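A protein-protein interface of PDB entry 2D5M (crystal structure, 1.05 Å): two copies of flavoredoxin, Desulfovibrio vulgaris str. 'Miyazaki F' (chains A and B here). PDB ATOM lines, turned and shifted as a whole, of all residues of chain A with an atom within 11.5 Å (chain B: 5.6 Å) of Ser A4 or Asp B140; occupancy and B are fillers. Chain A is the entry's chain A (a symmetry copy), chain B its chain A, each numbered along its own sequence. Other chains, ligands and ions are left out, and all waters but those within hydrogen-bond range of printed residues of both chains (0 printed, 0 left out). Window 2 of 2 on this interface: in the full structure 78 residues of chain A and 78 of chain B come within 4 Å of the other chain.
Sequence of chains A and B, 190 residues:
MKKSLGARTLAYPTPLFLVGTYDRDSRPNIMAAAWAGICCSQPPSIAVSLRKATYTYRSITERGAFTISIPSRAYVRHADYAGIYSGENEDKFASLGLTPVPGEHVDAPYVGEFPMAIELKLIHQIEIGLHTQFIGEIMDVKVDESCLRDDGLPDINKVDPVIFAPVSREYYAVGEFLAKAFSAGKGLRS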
ATOM      1  N   MET A   1      -0.871  -6.483  33.536  1.00  0.00           N
ATOM      2  CA  MET A   1      -1.304  -5.086  33.486  1.00  0.00           C
ATOM      3  C   MET A   1      -2.373  -4.757  32.425  1.00  0.00           C
ATOM      4  O   MET A   1      -2.115  -5.266  31.328  1.00  0.00           O
ATOM      5  CB  MET A   1      -0.115  -4.168  33.225  1.00  0.00           C
ATOM      6  CG  MET A   1      -0.706  -2.778  33.428  1.00  0.00           C
ATOM      7  SD  MET A   1      -0.660  -2.145  35.049  1.00  0.00           S
ATOM      8  CE  MET A   1       0.914  -2.352  35.844  1.00  0.00           C
ATOM      9  N   LYS A   2      -3.400  -3.951  32.692  1.00  0.00           N
ATOM     10  CA  LYS A   2      -4.371  -3.546  31.669  1.00  0.00           C
ATOM     11  C   LYS A   2      -4.009  -2.259  30.958  1.00  0.00           C
ATOM     12  O   LYS A   2      -3.369  -1.374  31.552  1.00  0.00           O
ATOM     13  CB  LYS A   2      -5.743  -3.355  32.333  1.00  0.00           C
ATOM     14  CG  LYS A   2      -6.236  -4.687  32.826  1.00  0.00           C
ATOM     15  CD  LYS A   2      -7.673  -4.941  32.790  1.00  0.00           C
ATOM     16  CE  LYS A   2      -8.158  -6.354  32.918  1.00  0.00           C
ATOM     17  NZ  LYS A   2      -7.377  -7.199  33.869  1.00  0.00           N
ATOM     18  N   LYS A   3      -4.390  -2.131  29.723  1.00  0.00           N
ATOM     19  CA  LYS A   3      -4.312  -0.910  28.934  1.00  0.00           C
ATOM     20  C   LYS A   3      -5.723  -0.401  28.675  1.00  0.00           C
ATOM     21  O   LYS A   3      -6.623  -1.185  28.369  1.00  0.00           O
ATOM     22  CB  LYS A   3      -3.562  -1.169  27.627  1.00  0.00           C
ATOM     23  CG  LYS A   3      -3.408   0.052  26.716  1.00  0.00           C
ATOM     24  CD  LYS A   3      -2.509  -0.280  25.529  1.00  0.00           C
ATOM     25  CE  LYS A   3      -2.003   0.948  24.816  1.00  0.00           C
ATOM     26  NZ  LYS A   3      -2.201   2.247  25.567  1.00  0.00           N
ATOM     27  N   SER A   4      -5.927   0.904  28.758  1.00  0.00           N
ATOM     28  CA  SER A   4      -7.174   1.538  28.401  1.00  0.00           C
ATOM     29  C   SER A   4      -7.269   1.754  26.886  1.00  0.00           C
ATOM     30  O   SER A   4      -6.362   2.333  26.272  1.00  0.00           O
ATOM     31  CB  SER A   4      -7.294   2.877  29.119  1.00  0.00           C
ATOM     32  OG  SER A   4      -8.238   3.706  28.494  1.00  0.00           O
ATOM     33  N   LEU A   5      -8.319   1.221  26.295  1.00  0.00           N
ATOM     34  CA  LEU A   5      -8.664   1.438  24.896  1.00  0.00           C
ATOM     35  C   LEU A   5      -9.669   2.564  24.693  1.00  0.00           C
ATOM     36  O   LEU A   5     -10.014   2.892  23.561  1.00  0.00           O
ATOM     37  CB  LEU A   5      -9.168   0.122  24.266  1.00  0.00           C
ATOM     38  CG  LEU A   5      -8.097  -0.829  23.793  1.00  0.00           C
ATOM     39  CD1 LEU A   5      -7.050  -1.201  24.833  1.00  0.00           C
ATOM     40  CD2 LEU A   5      -8.707  -2.105  23.205  1.00  0.00           C
ATOM     41  N   GLY A   6     -10.164   3.173  25.777  1.00  0.00           N
ATOM     42  CA  GLY A   6     -11.090   4.284  25.682  1.00  0.00           C
ATOM     43  C   GLY A   6     -12.542   3.794  25.505  1.00  0.00           C
ATOM     44  O   GLY A   6     -12.876   2.646  25.724  1.00  0.00           O
ATOM     45  N   ALA A   7     -13.389   4.739  25.133  1.00  0.00           N
ATOM     46  CA  ALA A   7     -14.813   4.516  25.083  1.00  0.00           C
ATOM     47  C   ALA A   7     -15.154   3.955  23.718  1.00  0.00           C
ATOM     48  O   ALA A   7     -15.398   4.697  22.756  1.00  0.00           O
ATOM     49  CB  ALA A   7     -15.520   5.809  25.382  1.00  0.00           C
ATOM     50  N   ARG A   8     -15.153   2.644  23.541  1.00  0.00           N
ATOM     51  CA  ARG A   8     -15.393   1.974  22.312  1.00  0.00           C
ATOM     52  C   ARG A   8     -16.466   0.928  22.467  1.00  0.00           C
ATOM     53  O   ARG A   8     -16.651   0.378  23.531  1.00  0.00           O
ATOM     54  CB  ARG A   8     -14.136   1.265  21.827  1.00  0.00           C
ATOM     55  CG  ARG A   8     -12.880   2.077  21.709  1.00  0.00           C
ATOM     56  CD  ARG A   8     -11.774   1.115  21.178  1.00  0.00           C
ATOM     57  NE  ARG A   8     -10.576   1.963  20.932  1.00  0.00           N
ATOM     58  CZ  ARG A   8     -10.188   2.436  19.766  1.00  0.00           C
ATOM     59  NH1 ARG A   8     -10.809   2.192  18.629  1.00  0.00           N
ATOM     60  NH2 ARG A   8      -9.105   3.199  19.633  1.00  0.00           N
ATOM     61  N   THR A   9     -17.171   0.618  21.367  1.00  0.00           N
ATOM     62  CA  THR A   9     -18.148  -0.452  21.327  1.00  0.00           C
ATOM     63  C   THR A   9     -17.432  -1.799  21.218  1.00  0.00           C
ATOM     64  O   THR A   9     -17.388  -2.409  20.120  1.00  0.00           O
ATOM     65  CB  THR A   9     -19.164  -0.288  20.177  1.00  0.00           C
ATOM     66  OG1 THR A   9     -18.431  -0.158  18.939  1.00  0.00           O
ATOM     67  CG2 THR A   9     -20.007   0.926  20.382  1.00  0.00           C
ATOM     68  N   LEU A  10     -16.860  -2.223  22.319  1.00  0.00           N
ATOM     69  CA  LEU A  10     -15.973  -3.372  22.354  1.00  0.00           C
ATOM     70  C   LEU A  10     -16.400  -4.302  23.466  1.00  0.00           C
ATOM     71  O   LEU A  10     -16.282  -3.986  24.638  1.00  0.00           O
ATOM     72  CB  LEU A  10     -14.571  -2.914  22.530  1.00  0.00           C
ATOM     73  CG  LEU A  10     -13.419  -3.839  22.366  1.00  0.00           C
ATOM     74  CD1 LEU A  10     -13.499  -4.725  21.148  1.00  0.00           C
ATOM     75  CD2 LEU A  10     -12.094  -2.997  22.322  1.00  0.00           C
ATOM     76  N   ALA A  11     -16.897  -5.463  23.086  1.00  0.00           N
ATOM     77  CA  ALA A  11     -17.305  -6.524  23.970  1.00  0.00           C
ATOM     78  C   ALA A  11     -17.330  -7.820  23.176  1.00  0.00           C
ATOM     79  O   ALA A  11     -17.446  -7.761  21.943  1.00  0.00           O
ATOM     80  CB  ALA A  11     -18.654  -6.263  24.599  1.00  0.00           C
ATOM     81  N   VAL A 167     -15.050  -3.573  16.164  1.00  0.00           N
ATOM     82  CA  VAL A 167     -13.921  -2.615  16.112  1.00  0.00           C
ATOM     83  C   VAL A 167     -12.781  -3.210  15.281  1.00  0.00           C
ATOM     84  O   VAL A 167     -12.377  -2.624  14.295  1.00  0.00           O
ATOM     85  CB  VAL A 167     -13.436  -2.107  17.474  1.00  0.00           C
ATOM     86  CG1 VAL A 167     -12.381  -1.035  17.291  1.00  0.00           C
ATOM     87  CG2 VAL A 167     -14.602  -1.579  18.300  1.00  0.00           C
ATOM     88  N   GLU B 104     -11.620   3.175  37.335  1.00  0.00           N
ATOM     89  CA  GLU B 104     -10.908   4.457  37.254  1.00  0.00           C
ATOM     90  C   GLU B 104     -11.840   5.584  36.904  1.00  0.00           C
ATOM     91  O   GLU B 104     -11.505   6.754  37.197  1.00  0.00           O
ATOM     92  CB  GLU B 104      -9.745   4.320  36.249  1.00  0.00           C
ATOM     93  CG  GLU B 104      -8.689   3.339  36.795  1.00  0.00           C
ATOM     94  CD  GLU B 104      -7.552   3.150  35.793  1.00  0.00           C
ATOM     95  OE1 GLU B 104      -7.902   3.087  34.560  1.00  0.00           O
ATOM     96  OE2 GLU B 104      -6.345   3.103  36.141  1.00  0.00           O
ATOM     97  N   HIS B 105     -12.952   5.290  36.228  1.00  0.00           N
ATOM     98  CA  HIS B 105     -13.853   6.272  35.686  1.00  0.00           C
ATOM     99  C   HIS B 105     -15.247   6.223  36.316  1.00  0.00           C
ATOM    100  O   HIS B 105     -16.001   7.183  36.194  1.00  0.00           O
ATOM    101  CB  HIS B 105     -13.987   6.103  34.161  1.00  0.00           C
ATOM    102  CG  HIS B 105     -12.678   6.178  33.459  1.00  0.00           C
ATOM    103  ND1 HIS B 105     -12.102   7.344  33.051  1.00  0.00           N
ATOM    104  CD2 HIS B 105     -11.809   5.156  33.145  1.00  0.00           C
ATOM    105  CE1 HIS B 105     -10.935   7.009  32.498  1.00  0.00           C
ATOM    106  NE2 HIS B 105     -10.726   5.715  32.541  1.00  0.00           N
ATOM    107  N   ALA B 117     -12.210  -5.691  30.879  1.00  0.00           N
ATOM    108  CA  ALA B 117     -13.167  -5.064  31.768  1.00  0.00           C
ATOM    109  C   ALA B 117     -13.659  -3.753  31.098  1.00  0.00           C
ATOM    110  O   ALA B 117     -12.907  -3.062  30.440  1.00  0.00           O
ATOM    111  CB  ALA B 117     -12.563  -4.783  33.117  1.00  0.00           C
ATOM    112  N   ILE B 118     -14.927  -3.483  31.297  1.00  0.00           N
ATOM    113  CA  ILE B 118     -15.602  -2.324  30.737  1.00  0.00           C
ATOM    114  C   ILE B 118     -16.208  -1.532  31.887  1.00  0.00           C
ATOM    115  O   ILE B 118     -16.867  -2.131  32.760  1.00  0.00           O
ATOM    116  CB  ILE B 118     -16.714  -2.793  29.749  1.00  0.00           C
ATOM    117  CG1 ILE B 118     -16.190  -3.769  28.721  1.00  0.00           C
ATOM    118  CG2 ILE B 118     -17.362  -1.567  29.130  1.00  0.00           C
ATOM    119  CD1 ILE B 118     -17.274  -4.394  27.861  1.00  0.00           C
ATOM    120  N   GLU B 119     -15.982  -0.233  31.925  1.00  0.00           N
ATOM    121  CA  GLU B 119     -16.534   0.651  32.928  1.00  0.00           C
ATOM    122  C   GLU B 119     -17.730   1.396  32.368  1.00  0.00           C
ATOM    123  O   GLU B 119     -17.593   2.038  31.308  1.00  0.00           O
ATOM    124  CB  GLU B 119     -15.461   1.668  33.389  1.00  0.00           C
ATOM    125  CG  GLU B 119     -14.248   1.027  34.015  1.00  0.00           C
ATOM    126  CD  GLU B 119     -13.424   1.976  34.856  1.00  0.00           C
ATOM    127  OE1 GLU B 119     -14.057   2.920  35.437  1.00  0.00           O
ATOM    128  OE2 GLU B 119     -12.202   1.731  34.974  1.00  0.00           O
ATOM    129  N   ILE B 138     -20.499   3.224  27.957  1.00  0.00           N
ATOM    130  CA  ILE B 138     -19.138   2.750  28.080  1.00  0.00           C
ATOM    131  C   ILE B 138     -18.194   3.936  28.207  1.00  0.00           C
ATOM    132  O   ILE B 138     -18.078   4.760  27.305  1.00  0.00           O
ATOM    133  CB  ILE B 138     -18.733   1.907  26.838  1.00  0.00           C
ATOM    134  CG1 ILE B 138     -19.625   0.678  26.702  1.00  0.00           C
ATOM    135  CG2 ILE B 138     -17.278   1.539  26.886  1.00  0.00           C
ATOM    136  CD1 ILE B 138     -19.459  -0.096  25.381  1.00  0.00           C
ATOM    137  N   MET B 139     -17.533   4.009  29.364  1.00  0.00           N
ATOM    138  CA  MET B 139     -16.587   5.061  29.674  1.00  0.00           C
ATOM    139  C   MET B 139     -15.170   4.646  29.370  1.00  0.00           C
ATOM    140  O   MET B 139     -14.303   5.515  29.094  1.00  0.00           O
ATOM    141  CB  MET B 139     -16.746   5.526  31.142  1.00  0.00           C
ATOM    142  CG  MET B 139     -18.151   5.865  31.538  1.00  0.00           C
ATOM    143  SD  MET B 139     -19.047   6.990  30.440  1.00  0.00           S
ATOM    144  CE  MET B 139     -18.117   8.475  30.711  1.00  0.00           C
ATOM    145  N   ASP B 140     -14.861   3.345  29.454  1.00  0.00           N
ATOM    146  CA  ASP B 140     -13.532   2.821  29.174  1.00  0.00           C
ATOM    147  C   ASP B 140     -13.636   1.343  28.993  1.00  0.00           C
ATOM    148  O   ASP B 140     -14.439   0.664  29.622  1.00  0.00           O
ATOM    149  CB  ASP B 140     -12.562   3.108  30.338  1.00  0.00           C
ATOM    150  CG  ASP B 140     -11.108   2.934  29.986  1.00  0.00           C
ATOM    151  OD1 ASP B 140     -10.735   3.106  28.805  1.00  0.00           O
ATOM    152  OD2 ASP B 140     -10.291   2.653  30.882  1.00  0.00           O
ATOM    153  N   VAL B 141     -12.808   0.816  28.118  1.00  0.00           N
ATOM    154  CA  VAL B 141     -12.583  -0.617  27.945  1.00  0.00           C
ATOM    155  C   VAL B 141     -11.095  -0.884  28.220  1.00  0.00           C
ATOM    156  O   VAL B 141     -10.226  -0.267  27.601  1.00  0.00           O
ATOM    157  CB  VAL B 141     -12.953  -1.040  26.518  1.00  0.00           C
ATOM    158  CG1 VAL B 141     -12.634  -2.538  26.358  1.00  0.00           C
ATOM    159  CG2 VAL B 141     -14.391  -0.696  26.172  1.00  0.00           C
ATOM    160  N   LYS B 142     -10.817  -1.756  29.166  1.00  0.00           N
ATOM    161  CA  LYS B 142      -9.487  -2.101  29.609  1.00  0.00           C
ATOM    162  C   LYS B 142      -9.183  -3.540  29.248  1.00  0.00           C
ATOM    163  O   LYS B 142      -9.989  -4.428  29.523  1.00  0.00           O
ATOM    164  CB  LYS B 142      -9.319  -1.918  31.136  1.00  0.00           C
ATOM    165  CG  LYS B 142      -9.211  -0.452  31.566  1.00  0.00           C
ATOM    166  CD  LYS B 142      -8.759  -0.407  33.026  1.00  0.00           C
ATOM    167  CE  LYS B 142      -9.707   0.362  33.890  1.00  0.00           C
ATOM    168  NZ  LYS B 142      -9.903   1.765  33.422  1.00  0.00           N
ATOM    169  N   VAL B 143      -8.026  -3.757  28.668  1.00  0.00           N
ATOM    170  CA  VAL B 143      -7.638  -5.122  28.217  1.00  0.00           C
ATOM    171  C   VAL B 143      -6.230  -5.381  28.650  1.00  0.00           C
ATOM    172  O   VAL B 143      -5.346  -4.544  28.528  1.00  0.00           O
ATOM    173  CB  VAL B 143      -7.817  -5.227  26.706  1.00  0.00           C
ATOM    174  CG1 VAL B 143      -7.379  -6.619  26.233  1.00  0.00           C
ATOM    175  CG2 VAL B 143      -9.252  -4.962  26.275  1.00  0.00           C
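Of the printed residues of chain B, Lys A3 touches Val B141 (3.8 Å), Lys B142 (3.3 Å) and Val B143 (2.9 Å).
Of the printed residues of chain B, Ser A4 touches Asp B140 (2.6 Å) and Val B141 (3.6 Å).
Ala B117 touches none of the printed residues of chain A.
No residue of chain A comes within 4 Å of Glu B119.
Of the printed residues of chain A, Ile B138 touches Ala A7 (3.4 Å) and Arg A8 (3.4 Å).
Met B139 touches just one residue of chain A: Ala A7 (3.9 Å).
Printed residues of chain A within 4 Å of Lys B142: Lys A2 (3.8 Å) and Lys A3 (3.3 Å).
Of the printed residues of chain A, Val B143 touches Lys A2 (3.4 Å) and Lys A3 (2.9 Å).
The nearest printed residue of chain B that does not touch Ser A4 is Lys B142 (4.3 Å).
The nearest printed residue of chain A that does not touch Asp B140 is Ala A7 (4.5 Å).
The nearest printed residue of chain B that does not touch Leu A5 is Val B143 (4.2 Å).
Among the printed residues, 16 pairs touch across the chains.
The side-chain carboxylate (OD1) of Asp B140 sits at hydrogen-bond distance from the side-chain hydroxyl (OG) of Ser A4, at 2.6 Å.
O of Val B141 sits at hydrogen-bond distance from N of Leu A5 (2.7 Å).
O of Val B143 sits at hydrogen-bond distance from N of Lys A3, at 2.9 Å.
The backbone carbonyl oxygen (O) of Gly A6 lies within hydrogen-bond range of the backbone NH (N) of Val B141.
The backbone NH of Gly A6 is in hydrogen-bond range of the side-chain carboxylate of Asp B140 (3.1 Å).
OG of Ser A4 sits at hydrogen-bond distance from N of Gly A6 (3.4 Å).
The backbone carbonyl oxygen (O) of Glu B119 sits at hydrogen-bond distance from the backbone NH (N) of Met B139 (2.8 Å).
N of Glu B119 is in hydrogen-bond range of O of Asp B140, at 2.9 Å.
The backbone carbonyl oxygen (O) of Leu A5 is in hydrogen-bond range of the guanidinium group (NE) of Arg A8 (2.8 Å).
The backbone carbonyl oxygen (O) of Ala B117 sits at hydrogen-bond distance from the backbone NH (N) of Lys B142 (2.8 Å).
NZ of Lys B142 lies within salt-bridge range of OD2 of Asp B140, at 2.7 Å.
CD of Lys A2 touches CB of Lys B142, at 3.8 Å.
Val B143 touches Lys A2 (O to CA, 3.4 Å).
O of Lys A3 touches O of Val B141, 3.8 Å away.
O of Lys A3 touches CA of Lys B142, 3.3 Å away.
Ser A4 touches Val B141 (CA to O, 3.6 Å).
Asp B140 touches Leu A5 (OD1 to N, 3.96 Å).
O of Met B139 touches CB of Ala A7, at 3.9 Å.
Ile B138 touches Arg A8.
Arg A8 touches Val B141.
Leu A10 touches Ile B118.
No position is printed for both chains.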
